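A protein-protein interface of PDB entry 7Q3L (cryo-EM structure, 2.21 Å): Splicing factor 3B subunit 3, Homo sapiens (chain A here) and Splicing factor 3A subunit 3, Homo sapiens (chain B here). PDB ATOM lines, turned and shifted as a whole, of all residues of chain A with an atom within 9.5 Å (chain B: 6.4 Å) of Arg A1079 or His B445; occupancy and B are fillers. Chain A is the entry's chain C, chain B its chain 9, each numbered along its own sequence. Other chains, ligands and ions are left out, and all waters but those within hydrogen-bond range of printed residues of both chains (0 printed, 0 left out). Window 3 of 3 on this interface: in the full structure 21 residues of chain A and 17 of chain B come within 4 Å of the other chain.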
ATOM      1  N   ILE A1023      -4.709   4.118   3.787  1.00  0.00           N
ATOM      2  CA  ILE A1023      -3.793   3.098   4.302  1.00  0.00           C
ATOM      3  C   ILE A1023      -3.283   2.246   3.137  1.00  0.00           C
ATOM      4  O   ILE A1023      -4.083   1.648   2.418  1.00  0.00           O
ATOM      5  CB  ILE A1023      -4.452   2.189   5.366  1.00  0.00           C
ATOM      6  CG1 ILE A1023      -4.895   2.962   6.611  1.00  0.00           C
ATOM      7  CG2 ILE A1023      -3.544   1.005   5.706  1.00  0.00           C
ATOM      8  CD1 ILE A1023      -5.689   2.138   7.610  1.00  0.00           C
ATOM      9  N   PHE A1024      -1.952   2.132   2.985  1.00  0.00           N
ATOM     10  CA  PHE A1024      -1.390   1.310   1.921  1.00  0.00           C
ATOM     11  C   PHE A1024      -0.580   0.105   2.420  1.00  0.00           C
ATOM     12  O   PHE A1024      -0.405  -0.838   1.655  1.00  0.00           O
ATOM     13  CB  PHE A1024      -0.635   2.159   0.897  1.00  0.00           C
ATOM     14  CG  PHE A1024       0.672   2.753   1.358  1.00  0.00           C
ATOM     15  CD1 PHE A1024       1.858   2.042   1.217  1.00  0.00           C
ATOM     16  CD2 PHE A1024       0.726   4.027   1.912  1.00  0.00           C
ATOM     17  CE1 PHE A1024       3.068   2.602   1.612  1.00  0.00           C
ATOM     18  CE2 PHE A1024       1.939   4.582   2.310  1.00  0.00           C
ATOM     19  CZ  PHE A1024       3.111   3.866   2.167  1.00  0.00           C
ATOM     20  N   VAL A1066      -2.291   4.261  -4.035  1.00  0.00           N
ATOM     21  CA  VAL A1066      -3.427   3.359  -3.845  1.00  0.00           C
ATOM     22  C   VAL A1066      -4.717   4.173  -3.693  1.00  0.00           C
ATOM     23  O   VAL A1066      -4.696   5.291  -3.189  1.00  0.00           O
ATOM     24  CB  VAL A1066      -3.184   2.392  -2.661  1.00  0.00           C
ATOM     25  CG1 VAL A1066      -4.396   1.543  -2.294  1.00  0.00           C
ATOM     26  CG2 VAL A1066      -2.003   1.477  -2.936  1.00  0.00           C
ATOM     27  N   ASP A1067      -5.847   3.571  -4.096  1.00  0.00           N
ATOM     28  CA  ASP A1067      -7.174   4.184  -4.084  1.00  0.00           C
ATOM     29  C   ASP A1067      -7.980   3.758  -2.852  1.00  0.00           C
ATOM     30  O   ASP A1067      -7.686   2.736  -2.243  1.00  0.00           O
ATOM     31  CB  ASP A1067      -7.953   3.755  -5.335  1.00  0.00           C
ATOM     32  CG  ASP A1067      -8.067   2.243  -5.482  1.00  0.00           C
ATOM     33  OD1 ASP A1067      -7.016   1.579  -5.576  1.00  0.00           O
ATOM     34  OD2 ASP A1067      -9.207   1.730  -5.449  1.00  0.00           O
ATOM     35  N   ASP A1069     -12.370   3.285  -2.475  1.00  0.00           N
ATOM     36  CA  ASP A1069     -13.487   3.324  -3.414  1.00  0.00           C
ATOM     37  C   ASP A1069     -14.610   4.276  -2.976  1.00  0.00           C
ATOM     38  O   ASP A1069     -15.093   4.181  -1.844  1.00  0.00           O
ATOM     39  CB  ASP A1069     -13.980   1.913  -3.736  1.00  0.00           C
ATOM     40  CG  ASP A1069     -15.122   1.871  -4.728  1.00  0.00           C
ATOM     41  OD1 ASP A1069     -16.269   2.133  -4.313  1.00  0.00           O
ATOM     42  OD2 ASP A1069     -14.880   1.508  -5.883  1.00  0.00           O
ATOM     43  N   GLY A1072     -17.951   2.068  -2.149  1.00  0.00           N
ATOM     44  CA  GLY A1072     -17.741   1.122  -1.061  1.00  0.00           C
ATOM     45  C   GLY A1072     -16.968  -0.149  -1.435  1.00  0.00           C
ATOM     46  O   GLY A1072     -16.664  -0.940  -0.537  1.00  0.00           O
ATOM     47  N   ASN A1073     -16.607  -0.341  -2.718  1.00  0.00           N
ATOM     48  CA  ASN A1073     -16.088  -1.618  -3.214  1.00  0.00           C
ATOM     49  C   ASN A1073     -14.848  -2.104  -2.454  1.00  0.00           C
ATOM     50  O   ASN A1073     -14.737  -3.303  -2.183  1.00  0.00           O
ATOM     51  CB  ASN A1073     -15.837  -1.579  -4.725  1.00  0.00           C
ATOM     52  CG  ASN A1073     -17.087  -1.276  -5.527  1.00  0.00           C
ATOM     53  OD1 ASN A1073     -18.094  -1.967  -5.398  1.00  0.00           O
ATOM     54  ND2 ASN A1073     -17.039  -0.240  -6.349  1.00  0.00           N
ATOM     55  N   LYS A1074     -13.934  -1.176  -2.101  1.00  0.00           N
ATOM     56  CA  LYS A1074     -12.672  -1.473  -1.418  1.00  0.00           C
ATOM     57  C   LYS A1074     -12.809  -1.762   0.086  1.00  0.00           C
ATOM     58  O   LYS A1074     -11.808  -1.922   0.792  1.00  0.00           O
ATOM     59  CB  LYS A1074     -11.643  -0.367  -1.673  1.00  0.00           C
ATOM     60  CG  LYS A1074     -10.359  -0.908  -2.276  1.00  0.00           C
ATOM     61  CD  LYS A1074      -9.273   0.128  -2.396  1.00  0.00           C
ATOM     62  CE  LYS A1074      -8.002  -0.397  -3.034  1.00  0.00           C
ATOM     63  NZ  LYS A1074      -8.200  -0.720  -4.468  1.00  0.00           N
ATOM     64  N   ALA A1075     -14.054  -1.835   0.570  1.00  0.00           N
ATOM     65  CA  ALA A1075     -14.404  -2.282   1.913  1.00  0.00           C
ATOM     66  C   ALA A1075     -15.439  -3.420   1.880  1.00  0.00           C
ATOM     67  O   ALA A1075     -15.992  -3.783   2.922  1.00  0.00           O
ATOM     68  CB  ALA A1075     -14.873  -1.086   2.710  1.00  0.00           C
ATOM     69  N   LEU A1076     -15.674  -4.002   0.683  1.00  0.00           N
ATOM     70  CA  LEU A1076     -16.706  -4.999   0.411  1.00  0.00           C
ATOM     71  C   LEU A1076     -16.154  -6.158  -0.425  1.00  0.00           C
ATOM     72  O   LEU A1076     -16.009  -7.270   0.092  1.00  0.00           O
ATOM     73  CB  LEU A1076     -17.898  -4.325  -0.283  1.00  0.00           C
ATOM     74  CG  LEU A1076     -18.879  -3.569   0.617  1.00  0.00           C
ATOM     75  CD1 LEU A1076     -19.951  -2.890  -0.222  1.00  0.00           C
ATOM     76  CD2 LEU A1076     -19.546  -4.509   1.614  1.00  0.00           C
ATOM     77  N   TRP A1077     -15.855  -5.888  -1.707  1.00  0.00           N
ATOM     78  CA  TRP A1077     -15.270  -6.857  -2.621  1.00  0.00           C
ATOM     79  C   TRP A1077     -13.746  -6.888  -2.456  1.00  0.00           C
ATOM     80  O   TRP A1077     -13.201  -7.853  -1.911  1.00  0.00           O
ATOM     81  CB  TRP A1077     -15.644  -6.515  -4.066  1.00  0.00           C
ATOM     82  CG  TRP A1077     -17.089  -6.319  -4.411  1.00  0.00           C
ATOM     83  CD1 TRP A1077     -17.704  -5.126  -4.655  1.00  0.00           C
ATOM     84  CD2 TRP A1077     -18.080  -7.342  -4.692  1.00  0.00           C
ATOM     85  NE1 TRP A1077     -19.005  -5.335  -5.039  1.00  0.00           N
ATOM     86  CE2 TRP A1077     -19.276  -6.686  -5.073  1.00  0.00           C
ATOM     87  CE3 TRP A1077     -18.092  -8.747  -4.657  1.00  0.00           C
ATOM     88  CZ2 TRP A1077     -20.439  -7.399  -5.425  1.00  0.00           C
ATOM     89  CZ3 TRP A1077     -19.242  -9.457  -4.977  1.00  0.00           C
ATOM     90  CH2 TRP A1077     -20.397  -8.782  -5.382  1.00  0.00           C
ATOM     91  N   ASP A1078     -13.090  -5.807  -2.910  1.00  0.00           N
ATOM     92  CA  ASP A1078     -11.656  -5.568  -2.812  1.00  0.00           C
ATOM     93  C   ASP A1078     -11.286  -5.252  -1.362  1.00  0.00           C
ATOM     94  O   ASP A1078     -12.086  -4.692  -0.618  1.00  0.00           O
ATOM     95  CB  ASP A1078     -11.242  -4.489  -3.817  1.00  0.00           C
ATOM     96  CG  ASP A1078      -9.747  -4.234  -3.926  1.00  0.00           C
ATOM     97  OD1 ASP A1078      -8.961  -5.080  -3.456  1.00  0.00           O
ATOM     98  OD2 ASP A1078      -9.380  -3.194  -4.501  1.00  0.00           O
ATOM     99  N   ARG A1079     -10.074  -5.681  -0.961  1.00  0.00           N
ATOM    100  CA  ARG A1079      -9.758  -5.899   0.445  1.00  0.00           C
ATOM    101  C   ARG A1079      -8.257  -6.075   0.698  1.00  0.00           C
ATOM    102  O   ARG A1079      -7.456  -6.282  -0.215  1.00  0.00           O
ATOM    103  CB  ARG A1079     -10.538  -7.116   0.976  1.00  0.00           C
ATOM    104  CG  ARG A1079     -10.412  -8.382   0.136  1.00  0.00           C
ATOM    105  CD  ARG A1079     -11.259  -9.521   0.692  1.00  0.00           C
ATOM    106  NE  ARG A1079     -12.640  -9.072   0.855  1.00  0.00           N
ATOM    107  CZ  ARG A1079     -13.435  -9.355   1.884  1.00  0.00           C
ATOM    108  NH1 ARG A1079     -14.670  -8.886   1.925  1.00  0.00           N
ATOM    109  NH2 ARG A1079     -13.021 -10.121   2.880  1.00  0.00           N
ATOM    110  N   GLY A1080      -7.897  -6.026   1.987  1.00  0.00           N
ATOM    111  CA  GLY A1080      -6.549  -6.299   2.469  1.00  0.00           C
ATOM    112  C   GLY A1080      -6.340  -7.759   2.878  1.00  0.00           C
ATOM    113  O   GLY A1080      -7.234  -8.596   2.763  1.00  0.00           O
ATOM    114  N   LEU A1081      -5.135  -8.040   3.381  1.00  0.00           N
ATOM    115  CA  LEU A1081      -4.642  -9.379   3.668  1.00  0.00           C
ATOM    116  C   LEU A1081      -4.651  -9.663   5.176  1.00  0.00           C
ATOM    117  O   LEU A1081      -4.197  -8.833   5.962  1.00  0.00           O
ATOM    118  CB  LEU A1081      -3.232  -9.445   3.073  1.00  0.00           C
ATOM    119  CG  LEU A1081      -2.481 -10.768   3.223  1.00  0.00           C
ATOM    120  CD1 LEU A1081      -3.222 -11.917   2.552  1.00  0.00           C
ATOM    121  CD2 LEU A1081      -1.070 -10.650   2.667  1.00  0.00           C
ATOM    122  N   LEU A1082      -5.176 -10.838   5.570  1.00  0.00           N
ATOM    123  CA  LEU A1082      -5.260 -11.340   6.946  1.00  0.00           C
ATOM    124  C   LEU A1082      -6.131 -10.484   7.882  1.00  0.00           C
ATOM    125  O   LEU A1082      -5.992 -10.612   9.100  1.00  0.00           O
ATOM    126  CB  LEU A1082      -3.861 -11.551   7.558  1.00  0.00           C
ATOM    127  CG  LEU A1082      -2.918 -12.520   6.841  1.00  0.00           C
ATOM    128  CD1 LEU A1082      -1.471 -12.189   7.173  1.00  0.00           C
ATOM    129  CD2 LEU A1082      -3.230 -13.969   7.179  1.00  0.00           C
ATOM    130  N   ASN A1083      -7.068  -9.683   7.341  1.00  0.00           N
ATOM    131  CA  ASN A1083      -7.818  -8.656   8.068  1.00  0.00           C
ATOM    132  C   ASN A1083      -7.011  -7.375   8.360  1.00  0.00           C
ATOM    133  O   ASN A1083      -7.485  -6.521   9.114  1.00  0.00           O
ATOM    134  CB  ASN A1083      -8.542  -9.192   9.315  1.00  0.00           C
ATOM    135  CG  ASN A1083      -9.297 -10.492   9.115  1.00  0.00           C
ATOM    136  OD1 ASN A1083     -10.229 -10.562   8.323  1.00  0.00           O
ATOM    137  ND2 ASN A1083      -8.939 -11.522   9.860  1.00  0.00           N
ATOM    138  N   GLY A1084      -5.831  -7.201   7.736  1.00  0.00           N
ATOM    139  CA  GLY A1084      -5.085  -5.943   7.696  1.00  0.00           C
ATOM    140  C   GLY A1084      -5.037  -5.347   6.285  1.00  0.00           C
ATOM    141  O   GLY A1084      -5.879  -5.688   5.459  1.00  0.00           O
ATOM    142  N   ALA A1085      -4.043  -4.494   5.983  1.00  0.00           N
ATOM    143  CA  ALA A1085      -3.845  -3.922   4.648  1.00  0.00           C
ATOM    144  C   ALA A1085      -3.386  -4.971   3.622  1.00  0.00           C
ATOM    145  O   ALA A1085      -2.966  -6.066   3.983  1.00  0.00           O
ATOM    146  CB  ALA A1085      -2.869  -2.766   4.732  1.00  0.00           C
ATOM    147  N   SER A1086      -3.440  -4.630   2.319  1.00  0.00           N
ATOM    148  CA  SER A1086      -3.078  -5.529   1.221  1.00  0.00           C
ATOM    149  C   SER A1086      -1.569  -5.779   1.103  1.00  0.00           C
ATOM    150  O   SER A1086      -1.158  -6.846   0.642  1.00  0.00           O
ATOM    151  CB  SER A1086      -3.639  -5.067  -0.108  1.00  0.00           C
ATOM    152  OG  SER A1086      -4.968  -4.603   0.024  1.00  0.00           O
ATOM    153  N   GLN A1087      -0.740  -4.794   1.487  1.00  0.00           N
ATOM    154  CA  GLN A1087       0.715  -4.899   1.451  1.00  0.00           C
ATOM    155  C   GLN A1087       1.251  -4.923   2.882  1.00  0.00           C
ATOM    156  O   GLN A1087       0.661  -4.299   3.756  1.00  0.00           O
ATOM    157  CB  GLN A1087       1.326  -3.713   0.700  1.00  0.00           C
ATOM    158  CG  GLN A1087       0.862  -3.567  -0.744  1.00  0.00           C
ATOM    159  CD  GLN A1087       1.348  -2.281  -1.379  1.00  0.00           C
ATOM    160  OE1 GLN A1087       2.134  -2.278  -2.330  1.00  0.00           O
ATOM    161  NE2 GLN A1087       0.884  -1.150  -0.873  1.00  0.00           N
ATOM    162  N   LYS A1088       2.353  -5.651   3.116  1.00  0.00           N
ATOM    163  CA  LYS A1088       2.875  -5.852   4.461  1.00  0.00           C
ATOM    164  C   LYS A1088       4.317  -5.372   4.569  1.00  0.00           C
ATOM    165  O   LYS A1088       5.099  -5.548   3.641  1.00  0.00           O
ATOM    166  CB  LYS A1088       2.824  -7.329   4.866  1.00  0.00           C
ATOM    167  CG  LYS A1088       1.426  -7.939   4.932  1.00  0.00           C
ATOM    168  CD  LYS A1088       0.474  -7.195   5.838  1.00  0.00           C
ATOM    169  CE  LYS A1088      -0.794  -7.979   6.096  1.00  0.00           C
ATOM    170  NZ  LYS A1088      -1.943  -7.093   6.373  1.00  0.00           N
ATOM    171  N   ASN B 442     -23.716  -9.361  -4.229  1.00  0.00           N
ATOM    172  CA  ASN B 442     -23.512 -10.671  -3.625  1.00  0.00           C
ATOM    173  C   ASN B 442     -22.098 -10.766  -3.044  1.00  0.00           C
ATOM    174  O   ASN B 442     -21.296 -11.571  -3.518  1.00  0.00           O
ATOM    175  CB  ASN B 442     -23.793 -11.809  -4.617  1.00  0.00           C
ATOM    176  CG  ASN B 442     -24.320 -13.076  -3.974  1.00  0.00           C
ATOM    177  OD1 ASN B 442     -24.814 -13.956  -4.679  1.00  0.00           O
ATOM    178  ND2 ASN B 442     -24.248 -13.168  -2.652  1.00  0.00           N
ATOM    179  N   THR B 443     -21.806  -9.968  -1.999  1.00  0.00           N
ATOM    180  CA  THR B 443     -20.490  -9.972  -1.358  1.00  0.00           C
ATOM    181  C   THR B 443     -20.375 -11.167  -0.408  1.00  0.00           C
ATOM    182  O   THR B 443     -21.397 -11.735  -0.042  1.00  0.00           O
ATOM    183  CB  THR B 443     -20.204  -8.643  -0.641  1.00  0.00           C
ATOM    184  OG1 THR B 443     -21.143  -8.488   0.423  1.00  0.00           O
ATOM    185  CG2 THR B 443     -20.279  -7.442  -1.557  1.00  0.00           C
ATOM    186  N   ALA B 444     -19.140 -11.538  -0.024  1.00  0.00           N
ATOM    187  CA  ALA B 444     -18.889 -12.616   0.925  1.00  0.00           C
ATOM    188  C   ALA B 444     -19.732 -12.448   2.193  1.00  0.00           C
ATOM    189  O   ALA B 444     -20.074 -13.436   2.844  1.00  0.00           O
ATOM    190  CB  ALA B 444     -17.415 -12.690   1.241  1.00  0.00           C
ATOM    191  N   HIS B 445     -20.071 -11.191   2.519  1.00  0.00           N
ATOM    192  CA  HIS B 445     -20.924 -10.873   3.659  1.00  0.00           C
ATOM    193  C   HIS B 445     -22.259 -11.629   3.590  1.00  0.00           C
ATOM    194  O   HIS B 445     -22.773 -12.036   4.629  1.00  0.00           O
ATOM    195  CB  HIS B 445     -21.158  -9.355   3.707  1.00  0.00           C
ATOM    196  CG  HIS B 445     -19.885  -8.592   3.799  1.00  0.00           C
ATOM    197  ND1 HIS B 445     -19.161  -8.200   2.695  1.00  0.00           N
ATOM    198  CD2 HIS B 445     -19.164  -8.223   4.874  1.00  0.00           C
ATOM    199  CE1 HIS B 445     -18.047  -7.629   3.103  1.00  0.00           C
ATOM    200  NE2 HIS B 445     -18.024  -7.624   4.432  1.00  0.00           N
ATOM    201  N   PHE B 446     -22.785 -11.862   2.376  1.00  0.00           N
ATOM    202  CA  PHE B 446     -24.057 -12.535   2.137  1.00  0.00           C
ATOM    203  C   PHE B 446     -23.912 -14.026   1.808  1.00  0.00           C
ATOM    204  O   PHE B 446     -24.919 -14.721   1.655  1.00  0.00           O
ATOM    205  CB  PHE B 446     -24.826 -11.804   1.037  1.00  0.00           C
ATOM    206  CG  PHE B 446     -25.032 -10.337   1.334  1.00  0.00           C
ATOM    207  CD1 PHE B 446     -26.063  -9.921   2.167  1.00  0.00           C
ATOM    208  CD2 PHE B 446     -24.186  -9.373   0.800  1.00  0.00           C
ATOM    209  CE1 PHE B 446     -26.262  -8.575   2.463  1.00  0.00           C
ATOM    210  CE2 PHE B 446     -24.376  -8.027   1.101  1.00  0.00           C
ATOM    211  CZ  PHE B 446     -25.415  -7.632   1.922  1.00  0.00           C
ATOM    212  N   ALA B 447     -22.685 -14.553   1.711  1.00  0.00           N
ATOM    213  CA  ALA B 447     -22.507 -16.002   1.675  1.00  0.00           C
ATOM    214  C   ALA B 447     -23.106 -16.622   2.941  1.00  0.00           C
ATOM    215  O   ALA B 447     -22.974 -16.058   4.021  1.00  0.00           O
ATOM    216  CB  ALA B 447     -21.043 -16.347   1.521  1.00  0.00           C
ATOM    217  N   ASN B 448     -23.764 -17.779   2.798  1.00  0.00           N
ATOM    218  CA  ASN B 448     -24.535 -18.473   3.828  1.00  0.00           C
ATOM    219  C   ASN B 448     -25.838 -17.766   4.270  1.00  0.00           C
ATOM    220  O   ASN B 448     -26.554 -18.336   5.102  1.00  0.00           O
ATOM    221  CB  ASN B 448     -23.637 -18.880   5.011  1.00  0.00           C
ATOM    222  CG  ASN B 448     -22.365 -19.603   4.607  1.00  0.00           C
ATOM    223  OD1 ASN B 448     -22.384 -20.486   3.758  1.00  0.00           O
ATOM    224  ND2 ASN B 448     -21.248 -19.276   5.228  1.00  0.00           N
ATOM    225  N   VAL B 449     -26.300 -16.714   3.559  1.00  0.00           N
ATOM    226  CA  VAL B 449     -27.595 -16.078   3.814  1.00  0.00           C
ATOM    227  C   VAL B 449     -28.643 -16.488   2.770  1.00  0.00           C
ATOM    228  O   VAL B 449     -28.541 -16.144   1.592  1.00  0.00           O
ATOM    229  CB  VAL B 449     -27.454 -14.545   3.915  1.00  0.00           C
ATOM    230  CG1 VAL B 449     -28.792 -13.812   3.943  1.00  0.00           C
ATOM    231  CG2 VAL B 449     -26.613 -14.153   5.116  1.00  0.00           C
ATOM    232  N   LEU B 458     -29.517  -7.184   6.749  1.00  0.00           N
ATOM    233  CA  LEU B 458     -28.063  -7.221   6.685  1.00  0.00           C
ATOM    234  C   LEU B 458     -27.523  -6.218   5.655  1.00  0.00           C
ATOM    235  O   LEU B 458     -26.552  -5.531   5.951  1.00  0.00           O
ATOM    236  CB  LEU B 458     -27.623  -8.666   6.417  1.00  0.00           C
ATOM    237  CG  LEU B 458     -26.125  -8.935   6.258  1.00  0.00           C
ATOM    238  CD1 LEU B 458     -25.338  -8.585   7.518  1.00  0.00           C
ATOM    239  CD2 LEU B 458     -25.896 -10.396   5.909  1.00  0.00           C
ATOM    240  N   LEU B 462     -25.035  -3.279   6.719  1.00  0.00           N
ATOM    241  CA  LEU B 462     -23.801  -3.171   5.949  1.00  0.00           C
ATOM    242  C   LEU B 462     -23.706  -1.847   5.193  1.00  0.00           C
ATOM    243  O   LEU B 462     -22.641  -1.248   5.183  1.00  0.00           O
ATOM    244  CB  LEU B 462     -23.674  -4.348   4.977  1.00  0.00           C
ATOM    245  CG  LEU B 462     -23.195  -5.666   5.580  1.00  0.00           C
ATOM    246  CD1 LEU B 462     -23.476  -6.797   4.614  1.00  0.00           C
ATOM    247  CD2 LEU B 462     -21.707  -5.621   5.897  1.00  0.00           C
ATOM    248  N   LYS B 466     -20.740   0.699   5.801  1.00  0.00           N
ATOM    249  CA  LYS B 466     -19.863   1.055   4.685  1.00  0.00           C
ATOM    250  C   LYS B 466     -20.040   2.498   4.192  1.00  0.00           C
ATOM    251  O   LYS B 466     -19.139   3.027   3.535  1.00  0.00           O
ATOM    252  CB  LYS B 466     -20.008   0.040   3.546  1.00  0.00           C
ATOM    253  CG  LYS B 466     -19.707  -1.404   3.933  1.00  0.00           C
ATOM    254  CD  LYS B 466     -18.247  -1.669   4.221  1.00  0.00           C
ATOM    255  CE  LYS B 466     -18.007  -2.832   5.160  1.00  0.00           C
ATOM    256  NZ  LYS B 466     -16.581  -2.889   5.555  1.00  0.00           N
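Arg A1079 touches just one residue of chain B: His B445.
Of chain A, only Leu A1076 and Arg A1079 come within 4 Å of His B445.
No residue of chain A comes within 4 Å of Phe B446.
Of the printed residues of chain B, Trp A1077 touches Asn B442 and Thr B443.
Printed residues of chain B within 4 Å of Ala A1075: Lys B466 (2.8 Å).
Printed residues of chain A within 4 Å of Lys B466: Ala A1075 and Leu A1076.
Of the printed residues of chain A, Asn B442 touches Trp A1077 (3.3 Å).
Val A1066 touches none of the printed residues of chain B.
The nearest residue of chain B that does not touch Arg A1079 is Ala B444 (4.7 Å).
The nearest printed residue of chain B that does not touch Ala A1075 is His B445 (4.4 Å).
Among the printed residues, merely in contact across the chains: Trp A1077 with Asn B442, Leu A1076 with His B445, Trp A1077 with Thr B443, Arg A1079 with His B445 and Leu A1076 with Lys B466.
Hydrophobic or aromatic side chains of chain A within 4 Å of the printed part of chain B: Ala A1075, Leu A1076 and Trp A1077.
The backbone carbonyl oxygen of Ala A1075 sits at hydrogen-bond distance from the side-chain amino group of Lys B466 (2.8 Å).
The backbone carbonyl oxygen of Leu A1076 sits at hydrogen-bond distance from the guanidinium group of Arg A1079, at 2.8 Å.
NE of Arg A1079 is in hydrogen-bond range of O of Trp A1077.
The backbone carbonyl oxygen (O) of Arg A1079 sits at hydrogen-bond distance from the side-chain hydroxyl (OG) of Ser A1086 (3.0 Å).
The side-chain hydroxyl (OG1) of Thr B443 lies within hydrogen-bond range of a ring nitrogen (ND1) of His B445.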
